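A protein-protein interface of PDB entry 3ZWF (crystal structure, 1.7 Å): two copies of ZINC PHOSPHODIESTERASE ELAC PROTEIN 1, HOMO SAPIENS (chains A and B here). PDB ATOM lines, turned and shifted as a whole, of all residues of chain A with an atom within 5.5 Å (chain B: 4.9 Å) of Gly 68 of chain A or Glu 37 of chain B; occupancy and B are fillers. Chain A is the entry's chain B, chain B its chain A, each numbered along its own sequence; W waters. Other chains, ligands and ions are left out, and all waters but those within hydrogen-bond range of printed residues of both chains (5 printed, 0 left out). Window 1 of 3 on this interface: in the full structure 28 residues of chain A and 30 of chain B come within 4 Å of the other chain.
The side-chain carboxylate (OE2) of Glu 37 of chain B lies within hydrogen-bond range of the backbone NH (N) of Gly 38 of chain A (2.7 Å). OE1 of Glu 37 of chain B is in hydrogen-bond range of NE2 of Gln 40 of chain A, 3.0 Å away. The side-chain carboxylate of Glu 37 of chain A sits at hydrogen-bond distance from the backbone NH of Gly 38 of chain B, at 2.6 Å.
The backbone NH of Gly 68 of chain B lies within hydrogen-bond range of the backbone carbonyl oxygen of Cys 35 of chain B (2.8 Å). The side-chain hydroxyl (OG1) of Thr 39 of chain B lies within hydrogen-bond range of the backbone carbonyl oxygen (O) of Gly 36 of chain B. O of Cys 35 of chain A sits at hydrogen-bond distance from N of Gly 68 of chain A, at 2.8 Å. The side-chain amide nitrogen (NE2) of Gln 40 of chain A lies close to the backbone carbonyl oxygen (O) of Gly 71 of chain A (3.4 Å).
Glu 37 of chain B touches Glu 37 of chain A (C to OE2, 3.5 Å). Glu 37 of chain A touches Thr 39 of chain B (OE2 to N, 3.99 Å). Glu 37 of chain A touches Gly 68 of chain B (OE2 to CA, 3.6 Å). Gln 40 of chain A touches Pro 13 of chain B. Gly 68 of chain A touches Glu 37 of chain B. Pro 70 of chain A touches Phe 67 of chain B (CB to CE2, 3.7 Å). OE1 of Glu 37 of chain B touches CA of Gly 71 of chain A (3.4 Å). N of Gly 71 of chain A touches CD2 of Phe 67 of chain B, at 3.7 Å.
Gly 68 of chain A touches just one residue of chain B: Glu 37 (3.6 Å). Printed residues of chain A within 4 Å of Glu 37 of chain B: Glu 37, Gly 38, Gln 40, Gly 68 and Gly 71. Printed residues of chain B within 4 Å of Gln 40 of chain A: Pro 13 (3.7 Å) and Glu 37 (3.0 Å). Of the printed residues of chain A, Phe 67 of chain B touches Pro 70 and Gly 71. Of the printed residues of chain B, Glu 37 of chain A touches Glu 37, Gly 38, Thr 39 and Gly 68. Printed residues of chain A within 4 Å of Pro 13 of chain B: Gln 40. Printed residues of chain A within 4 Å of Gly 68 of chain B: Glu 37. Cys 35 of chain A touches none of the printed residues of chain B. Leu 69 of chain A touches none of the printed residues of chain B. The nearest printed residue of chain B that does not touch Gly 68 of chain A is Phe 67 of chain B (6.6 Å). The nearest printed residue of chain A that does not touch Thr 39 of chain B is Gly 38 of chain A (7.7 Å).
Hydrophobic or aromatic side chains of chain A that line the printed part of chain B: Pro 70. Of the 10 printed residues of chain B, 6 touch a printed residue of chain A. Hydrophobic or aromatic side chains of chain B within 4 Å of the printed part of chain A: Pro 13 and Phe 67. Among the printed residues, no Asp or Glu carboxylate lies within 4 Å of a Lys or Arg side-chain nitrogen of the other chain.
Glu 37 of chain A touches its own counterpart, Glu 37 of chain B. Glu 37 of chain A touches Gly 38 of chain B, and with the chains exchanged Gly 38 of chain A touches Glu 37 of chain B. Glu 37 of chain A touches Thr 39 of chain B, but with the chains exchanged Thr 39 of chain A does not touch Glu 37 of chain B (4.01 Å). Glu 37 of chain A touches Gly 68 of chain B, and with the chains exchanged Gly 68 of chain A touches Glu 37 of chain B. Positions printed for both chains: 35, 36, 37, 38, 39, 63, 67 and 68. Of the 11 pairs that touch across the chains among the printed residues, 5 have their exchanged pair printed and touching as well.
Water W3 lies within hydrogen-bond range of the side-chain carboxylate (OE2) of Glu 37 of chain A, the backbone carbonyl oxygen (O) of Gly 68 of chain B and the backbone NH (N) of Thr 39 of chain B. Water W1 lies within hydrogen-bond range of OE2 of Glu 37 of chain B (2.7 Å), O of Gly 68 of chain A (2.8 Å), N of Gln 40 of chain A (2.8 Å) and N of Thr 39 of chain A (3.4 Å). Water W4 lies within hydrogen-bond range of OE1 of Glu 37 of chain B (2.8 Å), N of Gly 71 of chain A (2.8 Å) and O of Phe 67 of chain A (2.8 Å). Water W5 bridges the side-chain carboxylate (OE1) of Glu 37 of chain A (2.8 Å) and the backbone carbonyl oxygen (O) of Phe 67 of chain B (2.9 Å). Water W2 lies within hydrogen-bond range of the backbone carbonyl oxygen of Phe 67 of chain B (3.0 Å) and the backbone carbonyl oxygen of Phe 67 of chain A (3.0 Å).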
ATOM      1  N   CYS A  35     -16.844  20.794  12.272  1.00  0.00           N
ATOM      2  CA  CYS A  35     -16.430  22.050  12.873  1.00  0.00           C
ATOM      3  C   CYS A  35     -15.815  22.974  11.827  1.00  0.00           C
ATOM      4  O   CYS A  35     -14.632  23.353  11.900  1.00  0.00           O
ATOM      5  CB  CYS A  35     -15.496  21.789  14.060  1.00  0.00           C
ATOM      6  SG  CYS A  35     -15.258  23.180  15.168  1.00  0.00           S
ATOM      7  N   GLY A  36     -16.615  23.370  10.860  1.00  0.00           N
ATOM      8  CA  GLY A  36     -16.213  24.424   9.940  1.00  0.00           C
ATOM      9  C   GLY A  36     -15.902  25.772  10.600  1.00  0.00           C
ATOM     10  O   GLY A  36     -16.241  26.048  11.755  1.00  0.00           O
ATOM     11  N   GLU A  37     -15.246  26.607   9.824  1.00  0.00           N
ATOM     12  CA  GLU A  37     -14.952  27.937  10.291  1.00  0.00           C
ATOM     13  C   GLU A  37     -16.219  28.669  10.743  1.00  0.00           C
ATOM     14  O   GLU A  37     -17.251  28.600  10.076  1.00  0.00           O
ATOM     15  CB  GLU A  37     -14.247  28.682   9.173  1.00  0.00           C
ATOM     16  CG  GLU A  37     -14.015  30.118   9.619  1.00  0.00           C
ATOM     17  CD  GLU A  37     -12.891  30.841   8.871  1.00  0.00           C
ATOM     18  OE1 GLU A  37     -12.335  30.347   7.884  1.00  0.00           O
ATOM     19  OE2 GLU A  37     -12.643  32.011   9.255  1.00  0.00           O
ATOM     20  N   GLY A  38     -16.170  29.320  11.911  1.00  0.00           N
ATOM     21  CA  GLY A  38     -17.293  30.006  12.477  1.00  0.00           C
ATOM     22  C   GLY A  38     -18.154  29.225  13.437  1.00  0.00           C
ATOM     23  O   GLY A  38     -19.092  29.779  13.970  1.00  0.00           O
ATOM     24  N   THR A  39     -17.857  27.930  13.591  1.00  0.00           N
ATOM     25  CA  THR A  39     -18.638  27.091  14.501  1.00  0.00           C
ATOM     26  C   THR A  39     -18.676  27.677  15.919  1.00  0.00           C
ATOM     27  O   THR A  39     -19.730  27.770  16.540  1.00  0.00           O
ATOM     28  CB  THR A  39     -18.170  25.655  14.459  1.00  0.00           C
ATOM     29  OG1 THR A  39     -18.360  25.166  13.113  1.00  0.00           O
ATOM     30  CG2 THR A  39     -18.903  24.798  15.493  1.00  0.00           C
ATOM     31  N   GLN A  40     -17.523  28.173  16.392  1.00  0.00           N
ATOM     32  CA  GLN A  40     -17.527  28.693  17.749  1.00  0.00           C
ATOM     33  C   GLN A  40     -18.500  29.888  17.941  1.00  0.00           C
ATOM     34  O   GLN A  40     -19.140  30.016  18.997  1.00  0.00           O
ATOM     35  CB  GLN A  40     -16.111  29.048  18.228  1.00  0.00           C
ATOM     36  CG  GLN A  40     -15.416  30.143  17.421  1.00  0.00           C
ATOM     37  CD  GLN A  40     -14.187  30.674  18.143  1.00  0.00           C
ATOM     38  OE1 GLN A  40     -14.301  31.204  19.258  1.00  0.00           O
ATOM     39  NE2 GLN A  40     -13.028  30.588  17.499  1.00  0.00           N
ATOM     40  N   GLY A  63     -11.805  21.759   4.533  1.00  0.00           N
ATOM     41  CA  GLY A  63     -11.768  22.858   5.487  1.00  0.00           C
ATOM     42  C   GLY A  63     -13.081  23.334   6.095  1.00  0.00           C
ATOM     43  O   GLY A  63     -13.125  23.736   7.266  1.00  0.00           O
ATOM     44  N   PHE A  66     -13.534  21.313   9.307  1.00  0.00           N
ATOM     45  CA  PHE A  66     -12.605  21.287  10.442  1.00  0.00           C
ATOM     46  C   PHE A  66     -11.802  22.555  10.721  1.00  0.00           C
ATOM     47  O   PHE A  66     -11.166  22.612  11.749  1.00  0.00           O
ATOM     48  CB  PHE A  66     -11.656  20.078  10.381  1.00  0.00           C
ATOM     49  CG  PHE A  66     -10.510  20.219   9.451  1.00  0.00           C
ATOM     50  CD1 PHE A  66     -10.659  19.962   8.096  1.00  0.00           C
ATOM     51  CD2 PHE A  66      -9.220  20.524   9.927  1.00  0.00           C
ATOM     52  CE1 PHE A  66      -9.604  20.111   7.239  1.00  0.00           C
ATOM     53  CE2 PHE A  66      -8.123  20.643   9.048  1.00  0.00           C
ATOM     54  CZ  PHE A  66      -8.328  20.423   7.701  1.00  0.00           C
ATOM     55  N   PHE A  67     -11.846  23.522   9.825  1.00  0.00           N
ATOM     56  CA  PHE A  67     -10.985  24.728  10.028  1.00  0.00           C
ATOM     57  C   PHE A  67     -11.391  25.511  11.271  1.00  0.00           C
ATOM     58  O   PHE A  67     -10.563  26.300  11.767  1.00  0.00           O
ATOM     59  CB  PHE A  67     -11.009  25.662   8.816  1.00  0.00           C
ATOM     60  CG  PHE A  67     -10.157  25.248   7.652  1.00  0.00           C
ATOM     61  CD1 PHE A  67      -9.202  24.236   7.718  1.00  0.00           C
ATOM     62  CD2 PHE A  67     -10.322  25.910   6.435  1.00  0.00           C
ATOM     63  CE1 PHE A  67      -8.428  23.921   6.605  1.00  0.00           C
ATOM     64  CE2 PHE A  67      -9.542  25.591   5.314  1.00  0.00           C
ATOM     65  CZ  PHE A  67      -8.618  24.603   5.398  1.00  0.00           C
ATOM     66  N   GLY A  68     -12.644  25.334  11.753  1.00  0.00           N
ATOM     67  CA  GLY A  68     -13.069  25.951  13.011  1.00  0.00           C
ATOM     68  C   GLY A  68     -12.579  25.280  14.282  1.00  0.00           C
ATOM     69  O   GLY A  68     -12.769  25.789  15.399  1.00  0.00           O
ATOM     70  N   LEU A  69     -11.963  24.130  14.138  1.00  0.00           N
ATOM     71  CA  LEU A  69     -11.536  23.344  15.310  1.00  0.00           C
ATOM     72  C   LEU A  69     -10.489  23.953  16.249  1.00  0.00           C
ATOM     73  O   LEU A  69     -10.681  23.988  17.467  1.00  0.00           O
ATOM     74  CB  LEU A  69     -11.198  21.878  14.885  1.00  0.00           C
ATOM     75  CG  LEU A  69     -11.042  20.930  16.062  1.00  0.00           C
ATOM     76  CD1 LEU A  69     -12.196  20.896  17.017  1.00  0.00           C
ATOM     77  CD2 LEU A  69     -10.808  19.525  15.403  1.00  0.00           C
ATOM     78  N   PRO A  70      -9.408  24.517  15.696  1.00  0.00           N
ATOM     79  CA  PRO A  70      -8.418  25.138  16.590  1.00  0.00           C
ATOM     80  C   PRO A  70      -9.036  26.280  17.393  1.00  0.00           C
ATOM     81  O   PRO A  70      -8.811  26.386  18.614  1.00  0.00           O
ATOM     82  CB  PRO A  70      -7.351  25.631  15.622  1.00  0.00           C
ATOM     83  CG  PRO A  70      -7.420  24.713  14.500  1.00  0.00           C
ATOM     84  CD  PRO A  70      -8.906  24.443  14.321  1.00  0.00           C
ATOM     85  N   GLY A  71      -9.801  27.132  16.705  1.00  0.00           N
ATOM     86  CA  GLY A  71     -10.496  28.252  17.350  1.00  0.00           C
ATOM     87  C   GLY A  71     -11.415  27.805  18.422  1.00  0.00           C
ATOM     88  O   GLY A  71     -11.392  28.348  19.512  1.00  0.00           O
ATOM     89  N   LEU A  72     -12.200  26.745  18.138  1.00  0.00           N
ATOM     90  CA  LEU A  72     -13.140  26.208  19.113  1.00  0.00           C
ATOM     91  C   LEU A  72     -12.425  25.718  20.377  1.00  0.00           C
ATOM     92  O   LEU A  72     -12.824  26.047  21.494  1.00  0.00           O
ATOM     93  CB  LEU A  72     -13.990  25.107  18.518  1.00  0.00           C
ATOM     94  CG  LEU A  72     -15.026  24.525  19.494  1.00  0.00           C
ATOM     95  CD1 LEU A  72     -16.031  25.580  20.011  1.00  0.00           C
ATOM     96  CD2 LEU A  72     -15.727  23.317  18.888  1.00  0.00           C
ATOM     97  N   LEU A  73     -11.366  24.928  20.218  1.00  0.00           N
ATOM     98  CA  LEU A  73     -10.631  24.442  21.392  1.00  0.00           C
ATOM     99  C   LEU A  73     -10.053  25.594  22.214  1.00  0.00           C
ATOM    100  O   LEU A  73     -10.114  25.606  23.454  1.00  0.00           O
ATOM    101  CB  LEU A  73      -9.499  23.499  20.967  1.00  0.00           C
ATOM    102  CG  LEU A  73      -9.930  22.168  20.251  1.00  0.00           C
ATOM    103  CD1 LEU A  73      -8.757  21.387  19.841  1.00  0.00           C
ATOM    104  CD2 LEU A  73     -10.810  21.312  21.141  1.00  0.00           C
ATOM    105  N   PRO B  13     -13.477  35.484  18.230  1.00  0.00           N
ATOM    106  CA  PRO B  13     -14.593  36.157  17.594  1.00  0.00           C
ATOM    107  C   PRO B  13     -15.850  35.965  18.386  1.00  0.00           C
ATOM    108  O   PRO B  13     -16.009  34.909  18.971  1.00  0.00           O
ATOM    109  CB  PRO B  13     -14.699  35.435  16.253  1.00  0.00           C
ATOM    110  CG  PRO B  13     -14.135  34.132  16.498  1.00  0.00           C
ATOM    111  CD  PRO B  13     -13.099  34.255  17.525  1.00  0.00           C
ATOM    112  N   ALA B  19     -13.103  38.529  15.295  1.00  0.00           N
ATOM    113  CA  ALA B  19     -11.684  38.478  15.580  1.00  0.00           C
ATOM    114  C   ALA B  19     -10.921  39.440  14.674  1.00  0.00           C
ATOM    115  O   ALA B  19     -11.417  39.898  13.630  1.00  0.00           O
ATOM    116  CB  ALA B  19     -11.166  37.079  15.424  1.00  0.00           C
ATOM    117  N   CYS B  35      -6.165  38.179  10.300  1.00  0.00           N
ATOM    118  CA  CYS B  35      -7.159  37.277   9.707  1.00  0.00           C
ATOM    119  C   CYS B  35      -7.639  36.245  10.718  1.00  0.00           C
ATOM    120  O   CYS B  35      -7.426  35.051  10.588  1.00  0.00           O
ATOM    121  CB  CYS B  35      -6.594  36.612   8.445  1.00  0.00           C
ATOM    122  SG  CYS B  35      -7.852  35.888   7.388  1.00  0.00           S
ATOM    123  N   GLY B  36      -8.228  36.728  11.781  1.00  0.00           N
ATOM    124  CA  GLY B  36      -8.912  35.835  12.745  1.00  0.00           C
ATOM    125  C   GLY B  36     -10.026  35.010  12.137  1.00  0.00           C
ATOM    126  O   GLY B  36     -10.533  35.295  11.036  1.00  0.00           O
ATOM    127  N   GLU B  37     -10.429  33.990  12.888  1.00  0.00           N
ATOM    128  CA  GLU B  37     -11.509  33.145  12.467  1.00  0.00           C
ATOM    129  C   GLU B  37     -12.754  33.982  12.187  1.00  0.00           C
ATOM    130  O   GLU B  37     -13.079  34.904  12.940  1.00  0.00           O
ATOM    131  CB  GLU B  37     -11.781  32.122  13.565  1.00  0.00           C
ATOM    132  CG  GLU B  37     -12.986  31.291  13.211  1.00  0.00           C
ATOM    133  CD  GLU B  37     -13.113  29.989  13.962  1.00  0.00           C
ATOM    134  OE1 GLU B  37     -12.278  29.630  14.810  1.00  0.00           O
ATOM    135  OE2 GLU B  37     -14.099  29.330  13.683  1.00  0.00           O
ATOM    136  N   GLY B  38     -13.415  33.699  11.073  1.00  0.00           N
ATOM    137  CA  GLY B  38     -14.597  34.438  10.644  1.00  0.00           C
ATOM    138  C   GLY B  38     -14.377  35.633   9.749  1.00  0.00           C
ATOM    139  O   GLY B  38     -15.335  36.268   9.293  1.00  0.00           O
ATOM    140  N   THR B  39     -13.123  35.961   9.510  1.00  0.00           N
ATOM    141  CA  THR B  39     -12.813  37.046   8.605  1.00  0.00           C
ATOM    142  C   THR B  39     -13.452  36.919   7.228  1.00  0.00           C
ATOM    143  O   THR B  39     -14.034  37.866   6.730  1.00  0.00           O
ATOM    144  CB  THR B  39     -11.302  37.265   8.491  1.00  0.00           C
ATOM    145  OG1 THR B  39     -10.796  37.609   9.784  1.00  0.00           O
ATOM    146  CG2 THR B  39     -10.999  38.388   7.489  1.00  0.00           C
ATOM    147  N   GLY B  63      -4.118  32.787  17.553  1.00  0.00           N
ATOM    148  CA  GLY B  63      -5.142  32.323  16.652  1.00  0.00           C
ATOM    149  C   GLY B  63      -6.197  33.328  16.210  1.00  0.00           C
ATOM    150  O   GLY B  63      -6.689  33.256  15.073  1.00  0.00           O
ATOM    151  N   PHE B  67      -6.131  32.310  12.426  1.00  0.00           N
ATOM    152  CA  PHE B  67      -6.854  31.050  12.215  1.00  0.00           C
ATOM    153  C   PHE B  67      -7.852  31.143  11.060  1.00  0.00           C
ATOM    154  O   PHE B  67      -8.273  30.094  10.542  1.00  0.00           O
ATOM    155  CB  PHE B  67      -7.590  30.567  13.476  1.00  0.00           C
ATOM    156  CG  PHE B  67      -6.740  29.900  14.509  1.00  0.00           C
ATOM    157  CD1 PHE B  67      -5.414  29.562  14.299  1.00  0.00           C
ATOM    158  CD2 PHE B  67      -7.287  29.655  15.749  1.00  0.00           C
ATOM    159  CE1 PHE B  67      -4.684  28.960  15.312  1.00  0.00           C
ATOM    160  CE2 PHE B  67      -6.543  29.047  16.761  1.00  0.00           C
ATOM    161  CZ  PHE B  67      -5.251  28.724  16.538  1.00  0.00           C
ATOM    162  N   GLY B  68      -8.277  32.344  10.692  1.00  0.00           N
ATOM    163  CA  GLY B  68      -9.133  32.558   9.521  1.00  0.00           C
ATOM    164  C   GLY B  68      -8.463  32.489   8.155  1.00  0.00           C
ATOM    165  O   GLY B  68      -9.131  32.537   7.112  1.00  0.00           O
HETATM  166  O   HOH W   1     -15.026  27.414  15.309  1.00  0.00           O
HETATM  167  O   HOH W   2      -7.802  27.194  11.044  1.00  0.00           O
HETATM  168  O   HOH W   3     -11.564  33.684   7.587  1.00  0.00           O
HETATM  169  O   HOH W   4     -10.229  27.940  14.063  1.00  0.00           O
HETATM  170  O   HOH W   5      -9.784  29.201   8.216  1.00  0.00           O
